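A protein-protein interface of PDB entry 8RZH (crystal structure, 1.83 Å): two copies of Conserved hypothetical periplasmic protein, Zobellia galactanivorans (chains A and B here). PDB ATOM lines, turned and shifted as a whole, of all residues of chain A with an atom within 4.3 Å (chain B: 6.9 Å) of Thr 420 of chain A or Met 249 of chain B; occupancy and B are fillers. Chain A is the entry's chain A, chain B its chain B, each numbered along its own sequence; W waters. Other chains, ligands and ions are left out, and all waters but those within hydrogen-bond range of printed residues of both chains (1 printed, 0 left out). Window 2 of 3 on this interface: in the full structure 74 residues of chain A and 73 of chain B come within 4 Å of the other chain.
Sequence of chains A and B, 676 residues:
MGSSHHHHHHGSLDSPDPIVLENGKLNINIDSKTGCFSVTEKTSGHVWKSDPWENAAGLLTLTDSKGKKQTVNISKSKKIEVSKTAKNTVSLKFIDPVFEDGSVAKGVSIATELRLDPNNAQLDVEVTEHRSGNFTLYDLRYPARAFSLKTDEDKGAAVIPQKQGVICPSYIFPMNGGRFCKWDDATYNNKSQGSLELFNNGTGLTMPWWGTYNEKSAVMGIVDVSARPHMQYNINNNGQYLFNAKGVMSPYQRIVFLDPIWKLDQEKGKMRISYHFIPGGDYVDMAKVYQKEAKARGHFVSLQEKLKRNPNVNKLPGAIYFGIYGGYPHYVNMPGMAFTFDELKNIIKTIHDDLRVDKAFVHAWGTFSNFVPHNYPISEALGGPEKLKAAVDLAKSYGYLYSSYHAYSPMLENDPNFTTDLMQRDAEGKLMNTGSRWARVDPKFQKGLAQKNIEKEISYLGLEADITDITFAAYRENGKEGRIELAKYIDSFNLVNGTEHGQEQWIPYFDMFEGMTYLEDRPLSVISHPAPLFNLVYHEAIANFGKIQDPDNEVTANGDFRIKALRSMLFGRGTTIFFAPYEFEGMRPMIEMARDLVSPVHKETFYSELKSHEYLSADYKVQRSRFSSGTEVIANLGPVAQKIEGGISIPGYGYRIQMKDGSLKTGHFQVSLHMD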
ATOM      1  N   GLU A 413      -2.192  24.674  -3.301  1.00  0.00           N
ATOM      2  CA  GLU A 413      -0.970  25.465  -3.454  1.00  0.00           C
ATOM      3  C   GLU A 413      -0.971  26.304  -4.719  1.00  0.00           C
ATOM      4  O   GLU A 413      -0.393  27.391  -4.742  1.00  0.00           O
ATOM      5  CB  GLU A 413       0.242  24.530  -3.528  1.00  0.00           C
ATOM      6  CG  GLU A 413       0.605  23.892  -2.246  1.00  0.00           C
ATOM      7  CD  GLU A 413      -0.065  22.586  -1.973  1.00  0.00           C
ATOM      8  OE1 GLU A 413      -1.188  22.291  -2.457  1.00  0.00           O
ATOM      9  OE2 GLU A 413       0.552  21.837  -1.199  1.00  0.00           O
ATOM     10  N   PHE A 418      -4.994  30.887  -2.567  1.00  0.00           N
ATOM     11  CA  PHE A 418      -4.600  30.062  -1.421  1.00  0.00           C
ATOM     12  C   PHE A 418      -4.411  30.924  -0.182  1.00  0.00           C
ATOM     13  O   PHE A 418      -3.732  31.948  -0.232  1.00  0.00           O
ATOM     14  CB  PHE A 418      -3.284  29.321  -1.705  1.00  0.00           C
ATOM     15  CG  PHE A 418      -2.807  28.497  -0.527  1.00  0.00           C
ATOM     16  CD1 PHE A 418      -3.239  27.190  -0.355  1.00  0.00           C
ATOM     17  CD2 PHE A 418      -1.968  29.062   0.438  1.00  0.00           C
ATOM     18  CE1 PHE A 418      -2.801  26.425   0.755  1.00  0.00           C
ATOM     19  CE2 PHE A 418      -1.529  28.317   1.552  1.00  0.00           C
ATOM     20  CZ  PHE A 418      -1.954  27.017   1.721  1.00  0.00           C
ATOM     21  N   THR A 419      -4.979  30.479   0.935  1.00  0.00           N
ATOM     22  CA  THR A 419      -4.703  31.056   2.242  1.00  0.00           C
ATOM     23  C   THR A 419      -4.809  29.953   3.287  1.00  0.00           C
ATOM     24  O   THR A 419      -5.570  29.009   3.120  1.00  0.00           O
ATOM     25  CB  THR A 419      -5.701  32.179   2.600  1.00  0.00           C
ATOM     26  OG1 THR A 419      -5.546  32.521   3.963  1.00  0.00           O
ATOM     27  CG2 THR A 419      -7.128  31.733   2.417  1.00  0.00           C
ATOM     28  N   THR A 420      -4.077  30.088   4.389  1.00  0.00           N
ATOM     29  CA  THR A 420      -4.270  29.130   5.484  1.00  0.00           C
ATOM     30  C   THR A 420      -5.414  29.542   6.426  1.00  0.00           C
ATOM     31  O   THR A 420      -5.639  28.863   7.435  1.00  0.00           O
ATOM     32  CB  THR A 420      -2.971  28.987   6.277  1.00  0.00           C
ATOM     33  OG1 THR A 420      -2.613  30.275   6.782  1.00  0.00           O
ATOM     34  CG2 THR A 420      -1.823  28.528   5.361  1.00  0.00           C
ATOM     35  N   ASP A 421      -6.134  30.635   6.119  1.00  0.00           N
ATOM     36  CA  ASP A 421      -7.172  31.149   7.028  1.00  0.00           C
ATOM     37  C   ASP A 421      -8.288  30.137   7.276  1.00  0.00           C
ATOM     38  O   ASP A 421      -8.852  30.095   8.374  1.00  0.00           O
ATOM     39  CB  ASP A 421      -7.784  32.448   6.486  1.00  0.00           C
ATOM     40  CG  ASP A 421      -6.835  33.619   6.554  1.00  0.00           C
ATOM     41  OD1 ASP A 421      -5.730  33.470   7.119  1.00  0.00           O
ATOM     42  OD2 ASP A 421      -7.219  34.706   6.071  1.00  0.00           O
ATOM     43  N   LEU A 422      -8.650  29.338   6.271  1.00  0.00           N
ATOM     44  CA  LEU A 422      -9.736  28.380   6.435  1.00  0.00           C
ATOM     45  C   LEU A 422      -9.257  26.987   6.821  1.00  0.00           C
ATOM     46  O   LEU A 422     -10.076  26.055   6.863  1.00  0.00           O
ATOM     47  CB  LEU A 422     -10.566  28.313   5.145  1.00  0.00           C
ATOM     48  CG  LEU A 422     -11.295  29.631   4.834  1.00  0.00           C
ATOM     49  CD1 LEU A 422     -12.187  29.467   3.637  1.00  0.00           C
ATOM     50  CD2 LEU A 422     -12.085  30.145   6.025  1.00  0.00           C
ATOM     51  N   MET A 423      -7.960  26.816   7.107  1.00  0.00           N
ATOM     52  CA  MET A 423      -7.424  25.523   7.524  1.00  0.00           C
ATOM     53  C   MET A 423      -7.590  25.342   9.031  1.00  0.00           C
ATOM     54  O   MET A 423      -7.645  26.311   9.784  1.00  0.00           O
ATOM     55  CB  MET A 423      -5.932  25.416   7.148  1.00  0.00           C
ATOM     56  CG  MET A 423      -5.768  25.351   5.638  1.00  0.00           C
ATOM     57  SD  MET A 423      -4.046  25.267   5.075  1.00  0.00           S
ATOM     58  CE  MET A 423      -3.561  23.683   5.753  1.00  0.00           C
ATOM     59  N   LEU A 431      -0.977  23.858  11.842  1.00  0.00           N
ATOM     60  CA  LEU A 431      -1.909  23.519  10.758  1.00  0.00           C
ATOM     61  C   LEU A 431      -2.079  22.010  10.592  1.00  0.00           C
ATOM     62  O   LEU A 431      -1.110  21.242  10.642  1.00  0.00           O
ATOM     63  CB  LEU A 431      -1.434  24.129   9.436  1.00  0.00           C
ATOM     64  CG  LEU A 431      -1.434  25.645   9.320  1.00  0.00           C
ATOM     65  CD1 LEU A 431      -0.695  26.079   8.001  1.00  0.00           C
ATOM     66  CD2 LEU A 431      -2.891  26.105   9.278  1.00  0.00           C
ATOM     67  N   THR A 434      -1.564  19.667   6.251  1.00  0.00           N
ATOM     68  CA  THR A 434      -0.606  20.318   5.374  1.00  0.00           C
ATOM     69  C   THR A 434      -0.148  19.357   4.283  1.00  0.00           C
ATOM     70  O   THR A 434       0.227  19.803   3.201  1.00  0.00           O
ATOM     71  CB  THR A 434       0.605  20.842   6.142  1.00  0.00           C
ATOM     72  OG1 THR A 434       1.168  19.768   6.904  1.00  0.00           O
ATOM     73  CG2 THR A 434       0.197  22.022   7.058  1.00  0.00           C
ATOM     74  N   ARG A 440      -8.203  20.299   3.197  1.00  0.00           N
ATOM     75  CA  ARG A 440      -7.582  21.303   4.060  1.00  0.00           C
ATOM     76  C   ARG A 440      -8.579  22.281   4.687  1.00  0.00           C
ATOM     77  O   ARG A 440      -8.298  22.810   5.757  1.00  0.00           O
ATOM     78  CB  ARG A 440      -6.539  22.116   3.267  1.00  0.00           C
ATOM     79  CG  ARG A 440      -5.163  21.409   3.187  1.00  0.00           C
ATOM     80  CD  ARG A 440      -4.179  22.207   2.387  1.00  0.00           C
ATOM     81  NE  ARG A 440      -2.930  21.448   2.237  1.00  0.00           N
ATOM     82  CZ  ARG A 440      -2.154  21.547   1.167  1.00  0.00           C
ATOM     83  NH1 ARG A 440      -2.531  22.350   0.159  1.00  0.00           N
ATOM     84  NH2 ARG A 440      -1.035  20.807   1.067  1.00  0.00           N
ATOM     85  N   ASN B 238       7.395  19.693  -3.679  1.00  0.00           N
ATOM     86  CA  ASN B 238       7.928  20.961  -3.185  1.00  0.00           C
ATOM     87  C   ASN B 238       8.504  20.860  -1.778  1.00  0.00           C
ATOM     88  O   ASN B 238       8.729  21.897  -1.144  1.00  0.00           O
ATOM     89  CB  ASN B 238       6.845  22.054  -3.197  1.00  0.00           C
ATOM     90  CG  ASN B 238       5.705  21.764  -2.203  1.00  0.00           C
ATOM     91  OD1 ASN B 238       5.739  20.778  -1.480  1.00  0.00           O
ATOM     92  ND2 ASN B 238       4.714  22.635  -2.169  1.00  0.00           N
ATOM     93  N   GLN B 240       7.028  19.574   0.971  1.00  0.00           N
ATOM     94  CA  GLN B 240       6.061  19.680   2.069  1.00  0.00           C
ATOM     95  C   GLN B 240       6.343  18.630   3.151  1.00  0.00           C
ATOM     96  O   GLN B 240       6.084  18.866   4.336  1.00  0.00           O
ATOM     97  CB  GLN B 240       4.636  19.502   1.505  1.00  0.00           C
ATOM     98  CG  GLN B 240       3.538  19.714   2.557  1.00  0.00           C
ATOM     99  CD  GLN B 240       3.620  21.065   3.249  1.00  0.00           C
ATOM    100  OE1 GLN B 240       3.560  22.118   2.607  1.00  0.00           O
ATOM    101  NE2 GLN B 240       3.744  21.043   4.571  1.00  0.00           N
ATOM    102  N   PHE B 243       8.023  19.731   6.259  1.00  0.00           N
ATOM    103  CA  PHE B 243       7.332  20.731   7.058  1.00  0.00           C
ATOM    104  C   PHE B 243       6.076  20.213   7.734  1.00  0.00           C
ATOM    105  O   PHE B 243       5.484  20.953   8.537  1.00  0.00           O
ATOM    106  CB  PHE B 243       6.960  21.944   6.184  1.00  0.00           C
ATOM    107  CG  PHE B 243       8.150  22.690   5.689  1.00  0.00           C
ATOM    108  CD1 PHE B 243       8.787  23.601   6.503  1.00  0.00           C
ATOM    109  CD2 PHE B 243       8.685  22.401   4.432  1.00  0.00           C
ATOM    110  CE1 PHE B 243       9.926  24.273   6.066  1.00  0.00           C
ATOM    111  CE2 PHE B 243       9.815  23.058   3.988  1.00  0.00           C
ATOM    112  CZ  PHE B 243      10.450  23.977   4.795  1.00  0.00           C
ATOM    113  N   GLY B 247       3.807  21.547  10.951  1.00  0.00           N
ATOM    114  CA  GLY B 247       2.488  22.105  10.649  1.00  0.00           C
ATOM    115  C   GLY B 247       2.524  23.451   9.953  1.00  0.00           C
ATOM    116  O   GLY B 247       1.745  24.347  10.306  1.00  0.00           O
ATOM    117  N   VAL B 248       3.401  23.617   8.960  1.00  0.00           N
ATOM    118  CA  VAL B 248       3.462  24.846   8.180  1.00  0.00           C
ATOM    119  C   VAL B 248       3.560  24.450   6.716  1.00  0.00           C
ATOM    120  O   VAL B 248       3.842  23.296   6.376  1.00  0.00           O
ATOM    121  CB  VAL B 248       4.658  25.753   8.558  1.00  0.00           C
ATOM    122  CG1 VAL B 248       4.596  26.224  10.037  1.00  0.00           C
ATOM    123  CG2 VAL B 248       5.934  25.004   8.282  1.00  0.00           C
ATOM    124  N   MET B 249       3.326  25.430   5.835  1.00  0.00           N
ATOM    125  CA  MET B 249       3.339  25.166   4.392  1.00  0.00           C
ATOM    126  C   MET B 249       4.758  25.320   3.861  1.00  0.00           C
ATOM    127  O   MET B 249       5.486  26.238   4.261  1.00  0.00           O
ATOM    128  CB  MET B 249       2.408  26.129   3.637  1.00  0.00           C
ATOM    129  CG  MET B 249       0.912  26.129   4.096  1.00  0.00           C
ATOM    130  SD  MET B 249       0.233  24.459   4.029  1.00  0.00           S
ATOM    131  CE  MET B 249       0.332  24.066   2.289  1.00  0.00           C
ATOM    132  N   SER B 250       5.134  24.446   2.933  1.00  0.00           N
ATOM    133  CA  SER B 250       6.458  24.537   2.328  1.00  0.00           C
ATOM    134  C   SER B 250       6.602  25.853   1.573  1.00  0.00           C
ATOM    135  O   SER B 250       5.693  26.233   0.813  1.00  0.00           O
ATOM    136  CB  SER B 250       6.680  23.401   1.331  1.00  0.00           C
ATOM    137  OG  SER B 250       7.920  23.623   0.659  1.00  0.00           O
ATOM    138  N   PRO B 251       7.735  26.545   1.718  1.00  0.00           N
ATOM    139  CA  PRO B 251       8.033  27.727   0.896  1.00  0.00           C
ATOM    140  C   PRO B 251       8.807  27.420  -0.380  1.00  0.00           C
ATOM    141  O   PRO B 251       9.200  28.354  -1.089  1.00  0.00           O
ATOM    142  CB  PRO B 251       8.895  28.564   1.847  1.00  0.00           C
ATOM    143  CG  PRO B 251       9.653  27.546   2.622  1.00  0.00           C
ATOM    144  CD  PRO B 251       8.767  26.310   2.741  1.00  0.00           C
ATOM    145  N   TYR B 252       9.064  26.156  -0.659  1.00  0.00           N
ATOM    146  CA  TYR B 252       9.945  25.768  -1.747  1.00  0.00           C
ATOM    147  C   TYR B 252       9.180  25.478  -3.036  1.00  0.00           C
ATOM    148  O   TYR B 252       7.962  25.283  -3.048  1.00  0.00           O
ATOM    149  CB  TYR B 252      10.726  24.530  -1.352  1.00  0.00           C
ATOM    150  CG  TYR B 252      11.543  24.689  -0.090  1.00  0.00           C
ATOM    151  CD1 TYR B 252      12.074  25.940   0.297  1.00  0.00           C
ATOM    152  CD2 TYR B 252      11.803  23.587   0.696  1.00  0.00           C
ATOM    153  CE1 TYR B 252      12.845  26.054   1.490  1.00  0.00           C
ATOM    154  CE2 TYR B 252      12.564  23.694   1.854  1.00  0.00           C
ATOM    155  CZ  TYR B 252      13.079  24.910   2.233  1.00  0.00           C
ATOM    156  OH  TYR B 252      13.806  24.927   3.392  1.00  0.00           O
HETATM  157  O   HOH W   1       2.848  22.641  -0.021  1.00  0.00           O
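No position is printed for both chains.
Of the 8 pairs that touch across the chains among the printed residues, none has its exchanged pair printed and touching as well.
Phe 418 of chain A touches Met 249 of chain B (CZ to CE, 3.8 Å).
CG of Met 249 of chain B touches CG2 of Thr 420 of chain A (3.9 Å).
Gln 240 of chain B touches Thr 434 of chain A (CG to O, 3.4 Å).
Gly 247 of chain B touches Thr 434 of chain A (C to CG2, 3.98 Å).
Val 248 of chain B touches Thr 434 of chain A (O to CG2, 3.9 Å).
SD of Met 249 of chain B touches CG2 of Thr 434 of chain A (3.9 Å).
CE of Met 249 of chain B touches CZ of Arg 440 of chain A, at 3.7 Å.
The backbone NH (N) of Leu 431 of chain A lies within hydrogen-bond range of the backbone carbonyl oxygen (O) of Gly 247 of chain B (3.2 Å).
Of the 9 printed residues of chain B, 4 touch a printed residue of chain A.
Printed residues of chain B that touch a printed residue of chain A: Gln 240, Gly 247, Val 248 and Met 249.
Among the printed residues, no Asp or Glu carboxylate lies within 4 Å of a Lys or Arg side-chain nitrogen of the other chain.
Printed residues of chain B within 4 Å of Thr 420 of chain A: Met 249 (3.9 Å).
Met 249 of chain B touches just these residues of chain A: Phe 418, Thr 420, Thr 434 and Arg 440.
Of the printed residues of chain B, Thr 434 of chain A touches Gln 240 (3.4 Å), Gly 247 (3.98 Å), Val 248 (3.9 Å) and Met 249 (3.9 Å).
Of the printed residues of chain A, Gly 247 of chain B touches Leu 431 (3.2 Å) and Thr 434 (3.98 Å).
Thr 419 of chain A touches none of the printed residues of chain B.
Asn 238 of chain B touches none of the printed residues of chain A.
The nearest printed residue of chain B that does not touch Thr 420 of chain A is Val 248 of chain B (6.9 Å).
The side-chain amide nitrogen of Gln 240 of chain B lies within hydrogen-bond range of the backbone carbonyl oxygen of Val 248 of chain B (2.9 Å).
The side-chain carboxylate (OE1) of Glu 413 of chain A is in salt-bridge range of the guanidinium group (NH1) of Arg 440 of chain A, at 2.9 Å.
O of Thr 434 of chain A is in hydrogen-bond range of NH2 of Arg 440 of chain A.
O of Phe 243 of chain B lies within hydrogen-bond range of N of Val 248 of chain B (3.4 Å).
OD1 of Asn 238 of chain B lies within hydrogen-bond range of N of Gln 240 of chain B.
OE1 of Gln 240 of chain B is in hydrogen-bond range of N of Ser 250 of chain B (2.8 Å).
Water W1 lies within hydrogen-bond range of OE2 of Glu 413 of chain A, OE1 of Gln 240 of chain B and ND2 of Asn 238 of chain B.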
